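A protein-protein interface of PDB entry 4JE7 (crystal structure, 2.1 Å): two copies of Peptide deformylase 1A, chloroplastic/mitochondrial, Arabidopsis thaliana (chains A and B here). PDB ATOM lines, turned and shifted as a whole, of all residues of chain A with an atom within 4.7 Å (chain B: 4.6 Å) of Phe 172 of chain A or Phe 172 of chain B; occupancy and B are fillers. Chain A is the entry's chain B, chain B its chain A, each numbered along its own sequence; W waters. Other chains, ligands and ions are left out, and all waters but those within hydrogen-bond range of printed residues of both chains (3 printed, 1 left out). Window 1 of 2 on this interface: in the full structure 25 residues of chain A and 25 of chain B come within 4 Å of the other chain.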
ATOM      1  N   SER A   9      19.542   1.177  16.835  1.00  0.00           N
ATOM      2  CA  SER A   9      20.122  -0.150  16.940  1.00  0.00           C
ATOM      3  C   SER A   9      19.920  -0.659  18.374  1.00  0.00           C
ATOM      4  O   SER A   9      20.083   0.087  19.345  1.00  0.00           O
ATOM      5  CB  SER A   9      21.615  -0.130  16.519  1.00  0.00           C
ATOM      6  OG  SER A   9      22.049  -1.389  16.011  1.00  0.00           O
ATOM      7  N   GLY A  10      19.558  -1.930  18.521  1.00  0.00           N
ATOM      8  CA  GLY A  10      19.283  -2.475  19.875  1.00  0.00           C
ATOM      9  C   GLY A  10      17.842  -2.937  20.046  1.00  0.00           C
ATOM     10  O   GLY A  10      17.561  -3.898  20.810  1.00  0.00           O
ATOM     11  N   HIS A  15      16.557  -6.316  14.119  1.00  0.00           N
ATOM     12  CA  HIS A  15      17.575  -7.393  14.103  1.00  0.00           C
ATOM     13  C   HIS A  15      16.929  -8.738  13.832  1.00  0.00           C
ATOM     14  O   HIS A  15      17.502  -9.781  14.126  1.00  0.00           O
ATOM     15  CB  HIS A  15      18.390  -7.406  15.436  1.00  0.00           C
ATOM     16  CG  HIS A  15      19.006  -6.078  15.761  1.00  0.00           C
ATOM     17  ND1 HIS A  15      20.034  -5.534  15.019  1.00  0.00           N
ATOM     18  CD2 HIS A  15      18.685  -5.151  16.697  1.00  0.00           C
ATOM     19  CE1 HIS A  15      20.326  -4.335  15.494  1.00  0.00           C
ATOM     20  NE2 HIS A  15      19.527  -4.083  16.517  1.00  0.00           N
ATOM     21  N   VAL A 114      21.792   4.047  13.387  1.00  0.00           N
ATOM     22  CA  VAL A 114      23.153   4.119  13.962  1.00  0.00           C
ATOM     23  C   VAL A 114      23.634   5.582  13.848  1.00  0.00           C
ATOM     24  O   VAL A 114      24.421   5.923  12.996  1.00  0.00           O
ATOM     25  CB  VAL A 114      24.167   3.212  13.217  1.00  0.00           C
ATOM     26  CG1 VAL A 114      25.524   3.221  13.963  1.00  0.00           C
ATOM     27  CG2 VAL A 114      23.650   1.817  13.046  1.00  0.00           C
ATOM     28  N   PHE A 117      27.859   7.960  13.042  1.00  0.00           N
ATOM     29  CA  PHE A 117      28.923   7.080  12.618  1.00  0.00           C
ATOM     30  C   PHE A 117      28.687   6.737  11.120  1.00  0.00           C
ATOM     31  O   PHE A 117      27.541   6.900  10.570  1.00  0.00           O
ATOM     32  CB  PHE A 117      29.000   5.816  13.497  1.00  0.00           C
ATOM     33  CG  PHE A 117      29.573   6.067  14.904  1.00  0.00           C
ATOM     34  CD1 PHE A 117      30.933   5.984  15.146  1.00  0.00           C
ATOM     35  CD2 PHE A 117      28.752   6.432  15.949  1.00  0.00           C
ATOM     36  CE1 PHE A 117      31.459   6.260  16.437  1.00  0.00           C
ATOM     37  CE2 PHE A 117      29.269   6.692  17.231  1.00  0.00           C
ATOM     38  CZ  PHE A 117      30.639   6.606  17.453  1.00  0.00           C
ATOM     39  N   ARG A 118      29.784   6.275  10.482  1.00  0.00           N
ATOM     40  CA  ARG A 118      29.809   5.836   9.093  1.00  0.00           C
ATOM     41  C   ARG A 118      30.850   4.763   9.013  1.00  0.00           C
ATOM     42  O   ARG A 118      31.671   4.654   9.906  1.00  0.00           O
ATOM     43  CB  ARG A 118      30.262   6.987   8.226  1.00  0.00           C
ATOM     44  CG  ARG A 118      29.497   8.334   8.390  1.00  0.00           C
ATOM     45  CD  ARG A 118      28.236   8.358   7.544  1.00  0.00           C
ATOM     46  NE  ARG A 118      27.618   9.683   7.498  1.00  0.00           N
ATOM     47  CZ  ARG A 118      26.699  10.150   8.352  1.00  0.00           C
ATOM     48  NH1 ARG A 118      26.239  11.378   8.190  1.00  0.00           N
ATOM     49  NH2 ARG A 118      26.234   9.423   9.367  1.00  0.00           N
ATOM     50  N   ALA A 119      30.816   3.941   7.967  1.00  0.00           N
ATOM     51  CA  ALA A 119      31.878   3.003   7.670  1.00  0.00           C
ATOM     52  C   ALA A 119      31.854   2.822   6.136  1.00  0.00           C
ATOM     53  O   ALA A 119      30.890   3.207   5.482  1.00  0.00           O
ATOM     54  CB  ALA A 119      31.636   1.650   8.395  1.00  0.00           C
ATOM     55  N   TYR A 163      24.488  -2.233   8.470  1.00  0.00           N
ATOM     56  CA  TYR A 163      25.742  -2.188   7.713  1.00  0.00           C
ATOM     57  C   TYR A 163      26.905  -2.445   8.630  1.00  0.00           C
ATOM     58  O   TYR A 163      27.916  -2.861   8.160  1.00  0.00           O
ATOM     59  CB  TYR A 163      25.951  -0.856   7.026  1.00  0.00           C
ATOM     60  CG  TYR A 163      26.297   0.264   7.992  1.00  0.00           C
ATOM     61  CD1 TYR A 163      25.308   1.074   8.549  1.00  0.00           C
ATOM     62  CD2 TYR A 163      27.632   0.550   8.275  1.00  0.00           C
ATOM     63  CE1 TYR A 163      25.634   2.149   9.455  1.00  0.00           C
ATOM     64  CE2 TYR A 163      27.962   1.576   9.097  1.00  0.00           C
ATOM     65  CZ  TYR A 163      26.963   2.368   9.679  1.00  0.00           C
ATOM     66  OH  TYR A 163      27.390   3.323  10.464  1.00  0.00           O
ATOM     67  N   VAL A 164      26.784  -2.191   9.941  1.00  0.00           N
ATOM     68  CA  VAL A 164      27.947  -2.434  10.838  1.00  0.00           C
ATOM     69  C   VAL A 164      28.466  -3.894  10.805  1.00  0.00           C
ATOM     70  O   VAL A 164      29.621  -4.183  11.220  1.00  0.00           O
ATOM     71  CB  VAL A 164      27.617  -2.111  12.279  1.00  0.00           C
ATOM     72  CG1 VAL A 164      27.364  -0.650  12.413  1.00  0.00           C
ATOM     73  CG2 VAL A 164      26.383  -2.885  12.720  1.00  0.00           C
ATOM     74  N   MET A 167      30.634  -4.172   7.188  1.00  0.00           N
ATOM     75  CA  MET A 167      31.532  -3.075   6.794  1.00  0.00           C
ATOM     76  C   MET A 167      32.962  -3.508   6.665  1.00  0.00           C
ATOM     77  O   MET A 167      33.390  -4.417   7.334  1.00  0.00           O
ATOM     78  CB  MET A 167      31.483  -1.975   7.841  1.00  0.00           C
ATOM     79  CG  MET A 167      31.774  -2.447   9.264  1.00  0.00           C
ATOM     80  SD  MET A 167      31.461  -1.077  10.438  1.00  0.00           S
ATOM     81  CE  MET A 167      32.000  -1.793  12.007  1.00  0.00           C
ATOM     82  N   VAL A 168      33.731  -2.788   5.872  1.00  0.00           N
ATOM     83  CA  VAL A 168      35.180  -3.058   5.753  1.00  0.00           C
ATOM     84  C   VAL A 168      35.842  -2.818   7.144  1.00  0.00           C
ATOM     85  O   VAL A 168      35.539  -1.817   7.831  1.00  0.00           O
ATOM     86  CB  VAL A 168      35.810  -2.209   4.584  1.00  0.00           C
ATOM     87  CG1 VAL A 168      37.354  -2.280   4.527  1.00  0.00           C
ATOM     88  CG2 VAL A 168      35.248  -2.711   3.244  1.00  0.00           C
ATOM     89  N   ARG A 170      38.274  -1.622  10.149  1.00  0.00           N
ATOM     90  CA  ARG A 170      39.129  -0.423  10.288  1.00  0.00           C
ATOM     91  C   ARG A 170      38.604   0.845   9.626  1.00  0.00           C
ATOM     92  O   ARG A 170      39.283   1.879   9.654  1.00  0.00           O
ATOM     93  CB  ARG A 170      40.618  -0.713   9.876  1.00  0.00           C
ATOM     94  CG  ARG A 170      41.231  -1.759  10.771  1.00  0.00           C
ATOM     95  CD  ARG A 170      42.725  -2.047  10.683  1.00  0.00           C
ATOM     96  NE  ARG A 170      42.844  -3.455  11.051  1.00  0.00           N
ATOM     97  CZ  ARG A 170      43.947  -4.175  11.210  1.00  0.00           C
ATOM     98  NH1 ARG A 170      43.817  -5.449  11.511  1.00  0.00           N
ATOM     99  NH2 ARG A 170      45.155  -3.663  11.105  1.00  0.00           N
ATOM    100  N   THR A 171      37.414   0.812   9.022  1.00  0.00           N
ATOM    101  CA  THR A 171      36.921   2.030   8.354  1.00  0.00           C
ATOM    102  C   THR A 171      35.813   2.737   9.161  1.00  0.00           C
ATOM    103  O   THR A 171      35.397   3.842   8.819  1.00  0.00           O
ATOM    104  CB  THR A 171      36.413   1.779   6.913  1.00  0.00           C
ATOM    105  OG1 THR A 171      35.184   1.034   6.941  1.00  0.00           O
ATOM    106  CG2 THR A 171      37.458   1.012   6.075  1.00  0.00           C
ATOM    107  N   PHE A 172      35.307   2.081  10.199  1.00  0.00           N
ATOM    108  CA  PHE A 172      34.192   2.636  10.977  1.00  0.00           C
ATOM    109  C   PHE A 172      34.620   3.949  11.647  1.00  0.00           C
ATOM    110  O   PHE A 172      35.736   4.032  12.094  1.00  0.00           O
ATOM    111  CB  PHE A 172      33.842   1.636  12.061  1.00  0.00           C
ATOM    112  CG  PHE A 172      32.603   2.006  12.884  1.00  0.00           C
ATOM    113  CD1 PHE A 172      32.732   2.382  14.221  1.00  0.00           C
ATOM    114  CD2 PHE A 172      31.311   1.953  12.312  1.00  0.00           C
ATOM    115  CE1 PHE A 172      31.592   2.683  14.960  1.00  0.00           C
ATOM    116  CE2 PHE A 172      30.175   2.282  13.059  1.00  0.00           C
ATOM    117  CZ  PHE A 172      30.335   2.597  14.387  1.00  0.00           C
ATOM    118  N   ARG A 173      33.748   4.949  11.770  1.00  0.00           N
ATOM    119  CA  ARG A 173      34.209   6.279  12.220  1.00  0.00           C
ATOM    120  C   ARG A 173      33.093   7.238  12.549  1.00  0.00           C
ATOM    121  O   ARG A 173      31.983   7.091  12.064  1.00  0.00           O
ATOM    122  CB  ARG A 173      35.097   6.941  11.141  1.00  0.00           C
ATOM    123  CG  ARG A 173      34.411   7.149   9.757  1.00  0.00           C
ATOM    124  CD  ARG A 173      35.425   7.687   8.804  1.00  0.00           C
ATOM    125  NE  ARG A 173      36.553   6.750   8.548  1.00  0.00           N
ATOM    126  CZ  ARG A 173      37.664   7.073   7.861  1.00  0.00           C
ATOM    127  NH1 ARG A 173      37.769   8.287   7.327  1.00  0.00           N
ATOM    128  NH2 ARG A 173      38.651   6.184   7.671  1.00  0.00           N
ATOM    129  N   SER B   9      37.116   7.011  16.871  1.00  0.00           N
ATOM    130  CA  SER B   9      37.106   6.190  15.693  1.00  0.00           C
ATOM    131  C   SER B   9      37.133   6.992  14.375  1.00  0.00           C
ATOM    132  O   SER B   9      36.360   7.931  14.188  1.00  0.00           O
ATOM    133  CB  SER B   9      35.844   5.304  15.711  1.00  0.00           C
ATOM    134  OG  SER B   9      36.126   4.038  15.131  1.00  0.00           O
ATOM    135  N   GLY B  10      38.011   6.600  13.467  1.00  0.00           N
ATOM    136  CA  GLY B  10      38.227   7.293  12.200  1.00  0.00           C
ATOM    137  C   GLY B  10      39.653   7.841  12.102  1.00  0.00           C
ATOM    138  O   GLY B  10      40.221   7.925  10.991  1.00  0.00           O
ATOM    139  N   HIS B  15      43.707   2.736  14.120  1.00  0.00           N
ATOM    140  CA  HIS B  15      43.408   1.714  13.095  1.00  0.00           C
ATOM    141  C   HIS B  15      44.678   1.106  12.479  1.00  0.00           C
ATOM    142  O   HIS B  15      44.606   0.379  11.481  1.00  0.00           O
ATOM    143  CB  HIS B  15      42.436   2.309  12.058  1.00  0.00           C
ATOM    144  CG  HIS B  15      41.135   2.767  12.670  1.00  0.00           C
ATOM    145  ND1 HIS B  15      40.808   4.100  12.844  1.00  0.00           N
ATOM    146  CD2 HIS B  15      40.134   2.068  13.249  1.00  0.00           C
ATOM    147  CE1 HIS B  15      39.638   4.206  13.441  1.00  0.00           C
ATOM    148  NE2 HIS B  15      39.210   2.982  13.712  1.00  0.00           N
ATOM    149  N   VAL B 114      34.446   4.840  20.606  1.00  0.00           N
ATOM    150  CA  VAL B 114      33.137   4.711  19.943  1.00  0.00           C
ATOM    151  C   VAL B 114      32.019   5.129  20.939  1.00  0.00           C
ATOM    152  O   VAL B 114      31.371   4.276  21.614  1.00  0.00           O
ATOM    153  CB  VAL B 114      32.859   3.276  19.507  1.00  0.00           C
ATOM    154  CG1 VAL B 114      31.541   3.207  18.750  1.00  0.00           C
ATOM    155  CG2 VAL B 114      34.046   2.677  18.715  1.00  0.00           C
ATOM    156  N   PHE B 117      27.580   3.590  22.027  1.00  0.00           N
ATOM    157  CA  PHE B 117      27.254   2.206  21.583  1.00  0.00           C
ATOM    158  C   PHE B 117      27.902   1.099  22.399  1.00  0.00           C
ATOM    159  O   PHE B 117      28.881   1.341  23.136  1.00  0.00           O
ATOM    160  CB  PHE B 117      27.584   2.044  20.083  1.00  0.00           C
ATOM    161  CG  PHE B 117      26.632   2.805  19.197  1.00  0.00           C
ATOM    162  CD1 PHE B 117      26.896   4.135  18.852  1.00  0.00           C
ATOM    163  CD2 PHE B 117      25.431   2.220  18.783  1.00  0.00           C
ATOM    164  CE1 PHE B 117      25.999   4.838  18.090  1.00  0.00           C
ATOM    165  CE2 PHE B 117      24.536   2.936  18.022  1.00  0.00           C
ATOM    166  CZ  PHE B 117      24.826   4.241  17.681  1.00  0.00           C
ATOM    167  N   ARG B 118      27.312  -0.097  22.306  1.00  0.00           N
ATOM    168  CA  ARG B 118      27.830  -1.288  22.940  1.00  0.00           C
ATOM    169  C   ARG B 118      27.645  -2.493  21.972  1.00  0.00           C
ATOM    170  O   ARG B 118      26.797  -2.481  21.097  1.00  0.00           O
ATOM    171  CB  ARG B 118      27.072  -1.549  24.260  1.00  0.00           C
ATOM    172  CG  ARG B 118      26.972  -0.356  25.289  1.00  0.00           C
ATOM    173  CD  ARG B 118      28.323  -0.220  26.044  1.00  0.00           C
ATOM    174  NE  ARG B 118      28.231   0.718  27.168  1.00  0.00           N
ATOM    175  CZ  ARG B 118      28.452   2.035  27.064  1.00  0.00           C
ATOM    176  NH1 ARG B 118      28.822   2.579  25.885  1.00  0.00           N
ATOM    177  NH2 ARG B 118      28.279   2.830  28.130  1.00  0.00           N
ATOM    178  N   ALA B 119      28.392  -3.566  22.164  1.00  0.00           N
ATOM    179  CA  ALA B 119      28.057  -4.817  21.474  1.00  0.00           C
ATOM    180  C   ALA B 119      28.615  -6.028  22.198  1.00  0.00           C
ATOM    181  O   ALA B 119      29.518  -5.885  23.023  1.00  0.00           O
ATOM    182  CB  ALA B 119      28.509  -4.781  20.011  1.00  0.00           C
ATOM    183  N   TYR B 163      36.586  -3.227  18.778  1.00  0.00           N
ATOM    184  CA  TYR B 163      35.621  -4.314  19.065  1.00  0.00           C
ATOM    185  C   TYR B 163      34.592  -4.441  17.924  1.00  0.00           C
ATOM    186  O   TYR B 163      34.140  -5.546  17.608  1.00  0.00           O
ATOM    187  CB  TYR B 163      34.957  -4.116  20.426  1.00  0.00           C
ATOM    188  CG  TYR B 163      33.819  -3.066  20.471  1.00  0.00           C
ATOM    189  CD1 TYR B 163      32.485  -3.435  20.223  1.00  0.00           C
ATOM    190  CD2 TYR B 163      34.082  -1.760  20.785  1.00  0.00           C
ATOM    191  CE1 TYR B 163      31.472  -2.514  20.271  1.00  0.00           C
ATOM    192  CE2 TYR B 163      33.074  -0.812  20.825  1.00  0.00           C
ATOM    193  CZ  TYR B 163      31.781  -1.184  20.563  1.00  0.00           C
ATOM    194  OH  TYR B 163      30.809  -0.234  20.594  1.00  0.00           O
ATOM    195  N   VAL B 164      34.281  -3.327  17.251  1.00  0.00           N
ATOM    196  CA  VAL B 164      33.193  -3.274  16.239  1.00  0.00           C
ATOM    197  C   VAL B 164      33.516  -4.212  15.099  1.00  0.00           C
ATOM    198  O   VAL B 164      32.625  -4.704  14.390  1.00  0.00           O
ATOM    199  CB  VAL B 164      32.851  -1.787  15.784  1.00  0.00           C
ATOM    200  CG1 VAL B 164      32.273  -0.965  16.980  1.00  0.00           C
ATOM    201  CG2 VAL B 164      34.037  -1.090  15.278  1.00  0.00           C
ATOM    202  N   MET B 167      32.627  -8.228  16.748  1.00  0.00           N
ATOM    203  CA  MET B 167      31.428  -8.324  17.618  1.00  0.00           C
ATOM    204  C   MET B 167      30.453  -9.322  17.033  1.00  0.00           C
ATOM    205  O   MET B 167      30.513  -9.651  15.812  1.00  0.00           O
ATOM    206  CB  MET B 167      30.756  -6.953  17.786  1.00  0.00           C
ATOM    207  CG  MET B 167      30.166  -6.352  16.472  1.00  0.00           C
ATOM    208  SD  MET B 167      29.641  -4.631  16.711  1.00  0.00           S
ATOM    209  CE  MET B 167      29.189  -4.197  15.047  1.00  0.00           C
ATOM    210  N   ARG B 170      24.363  -8.635  14.875  1.00  0.00           N
ATOM    211  CA  ARG B 170      23.008  -8.329  15.339  1.00  0.00           C
ATOM    212  C   ARG B 170      22.911  -7.925  16.781  1.00  0.00           C
ATOM    213  O   ARG B 170      21.804  -7.957  17.348  1.00  0.00           O
ATOM    214  CB  ARG B 170      22.010  -9.502  15.074  1.00  0.00           C
ATOM    215  CG  ARG B 170      21.826  -9.821  13.585  1.00  0.00           C
ATOM    216  CD  ARG B 170      20.654 -10.710  13.263  1.00  0.00           C
ATOM    217  NE  ARG B 170      21.094 -11.653  12.232  1.00  0.00           N
ATOM    218  CZ  ARG B 170      20.653 -11.686  10.983  1.00  0.00           C
ATOM    219  NH1 ARG B 170      21.125 -12.570  10.104  1.00  0.00           N
ATOM    220  NH2 ARG B 170      19.722 -10.839  10.612  1.00  0.00           N
ATOM    221  N   THR B 171      24.035  -7.563  17.406  1.00  0.00           N
ATOM    222  CA  THR B 171      24.027  -7.156  18.850  1.00  0.00           C
ATOM    223  C   THR B 171      24.437  -5.676  19.064  1.00  0.00           C
ATOM    224  O   THR B 171      24.304  -5.138  20.159  1.00  0.00           O
ATOM    225  CB  THR B 171      24.885  -8.124  19.782  1.00  0.00           C
ATOM    226  OG1 THR B 171      26.276  -7.958  19.512  1.00  0.00           O
ATOM    227  CG2 THR B 171      24.516  -9.619  19.579  1.00  0.00           C
ATOM    228  N   PHE B 172      24.953  -5.015  18.032  1.00  0.00           N
ATOM    229  CA  PHE B 172      25.380  -3.628  18.185  1.00  0.00           C
ATOM    230  C   PHE B 172      24.166  -2.816  18.664  1.00  0.00           C
ATOM    231  O   PHE B 172      23.062  -2.980  18.134  1.00  0.00           O
ATOM    232  CB  PHE B 172      25.871  -3.128  16.819  1.00  0.00           C
ATOM    233  CG  PHE B 172      26.630  -1.816  16.853  1.00  0.00           C
ATOM    234  CD1 PHE B 172      27.865  -1.722  17.469  1.00  0.00           C
ATOM    235  CD2 PHE B 172      26.123  -0.721  16.213  1.00  0.00           C
ATOM    236  CE1 PHE B 172      28.569  -0.536  17.451  1.00  0.00           C
ATOM    237  CE2 PHE B 172      26.833   0.474  16.167  1.00  0.00           C
ATOM    238  CZ  PHE B 172      28.063   0.561  16.783  1.00  0.00           C
ATOM    239  N   ARG B 173      24.334  -1.968  19.668  1.00  0.00           N
ATOM    240  CA  ARG B 173      23.155  -1.249  20.178  1.00  0.00           C
ATOM    241  C   ARG B 173      23.558   0.087  20.762  1.00  0.00           C
ATOM    242  O   ARG B 173      24.724   0.255  21.076  1.00  0.00           O
ATOM    243  CB  ARG B 173      22.425  -2.102  21.225  1.00  0.00           C
ATOM    244  CG  ARG B 173      23.342  -2.725  22.304  1.00  0.00           C
ATOM    245  CD  ARG B 173      22.524  -3.711  23.156  1.00  0.00           C
ATOM    246  NE  ARG B 173      21.943  -4.725  22.298  1.00  0.00           N
ATOM    247  CZ  ARG B 173      21.016  -5.594  22.640  1.00  0.00           C
ATOM    248  NH1 ARG B 173      20.504  -5.613  23.867  1.00  0.00           N
ATOM    249  NH2 ARG B 173      20.609  -6.445  21.721  1.00  0.00           N
HETATM  250  O   HOH W   1      41.486   5.973   9.514  1.00  0.00           O
HETATM  251  O   HOH W   2      17.929  -6.757  20.048  1.00  0.00           O
HETATM  252  O   HOH W   3      45.998  -0.870   9.664  1.00  0.00           O
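A ring nitrogen (NE2) of His 15 of chain A sits at hydrogen-bond distance from the backbone NH of Gly 10 of chain A, 2.9 Å away.
The backbone NH of Arg 173 of chain A is in hydrogen-bond range of the backbone carbonyl oxygen of Arg 118 of chain A (2.8 Å).
The guanidinium group (NE) of Arg 173 of chain A is in hydrogen-bond range of the backbone carbonyl oxygen (O) of Thr 171 of chain A (3.1 Å).
NE of Arg 173 of chain B is in hydrogen-bond range of O of Thr 171 of chain B, at 3.2 Å.
The backbone carbonyl oxygen (O) of Arg 173 of chain B sits at hydrogen-bond distance from the backbone NH (N) of Arg 118 of chain B.
O of Phe 172 of chain B lies within hydrogen-bond range of OG of Ser 9 of chain A (2.8 Å).
O of Phe 172 of chain A sits at hydrogen-bond distance from OG of Ser 9 of chain B (3.1 Å).
Of the 15 printed residues of chain A, 10 touch a printed residue of chain B.
Hydrophobic or aromatic side chains of chain B that line the printed part of chain A: His 15, Val 114, Phe 117, Val 164, Met 167 and Phe 172.
Among the printed residues, no Asp or Glu carboxylate lies within 4 Å of a Lys or Arg side-chain nitrogen of the other chain.
Of the printed residues of chain B, Ser 9 of chain A touches Phe 172 (2.8 Å) and Arg 173 (3.5 Å).
Printed residues of chain B within 4 Å of Met 167 of chain A: Val 164 (3.8 Å).
Thr 171 of chain A touches none of the printed residues of chain B.
Phe 172 of chain A touches six residues of chain B.
Arg 118 of chain B touches none of the printed residues of chain A.
Phe 172 of chain B touches five residues of chain A.
The nearest printed residue of chain B that does not touch Phe 172 of chain A is Phe 117 of chain B (5.8 Å).
The nearest printed residue of chain A that does not touch Gly 10 of chain B is Thr 171 of chain A (5.6 Å).
Ser 9 of chain A touches Arg 173 of chain B, and with the chains exchanged Arg 173 of chain A touches Ser 9 of chain B.
Gly 10 of chain A touches Arg 173 of chain B, and with the chains exchanged Arg 173 of chain A touches Gly 10 of chain B.
His 15 of chain A touches Arg 170 of chain B, and with the chains exchanged Arg 170 of chain A touches His 15 of chain B.
Phe 172 of chain A touches His 15 of chain B, but with the chains exchanged His 15 of chain A does not touch Phe 172 of chain B (4.04 Å).
Positions printed for both chains: 9, 10, 15, 114, 117, 118, 119, 163, 164, 167, 170, 171, 172 and 173.
Of the 21 pairs that touch across the chains among the printed residues, 20 have their exchanged pair printed and touching as well.
Water W3 lies within hydrogen-bond range of O of His 15 of chain B (2.6 Å) and NH2 of Arg 170 of chain A (3.3 Å).
Water W1 bridges the backbone carbonyl oxygen (O) of Gly 10 of chain B (2.8 Å) and the guanidinium group (NH2) of Arg 173 of chain A (3.4 Å).
Water W2 bridges the backbone carbonyl oxygen of Gly 10 of chain A (3.0 Å) and the guanidinium group of Arg 173 of chain B (3.2 Å).
CA of Arg 173 of chain B touches O of Ser 9 of chain A, 3.5 Å away.
Gly 10 of chain A touches Phe 172 of chain B.
Gly 10 of chain A touches Arg 173 of chain B.
CD of Arg 170 of chain B touches O of His 15 of chain A, at 3.4 Å.
Val 114 of chain B touches Phe 117 of chain A (CG1 to CZ, 3.7 Å).
CD2 of Phe 117 of chain A touches CE1 of Phe 117 of chain B, at 3.8 Å.
N of Gly 10 of chain B touches O of Phe 172 of chain A, at 3.7 Å.
Phe 172 of chain A touches His 15 of chain B.
Val 114 of chain B touches Phe 172 of chain A.
Phe 172 of chain A touches Val 164 of chain B.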
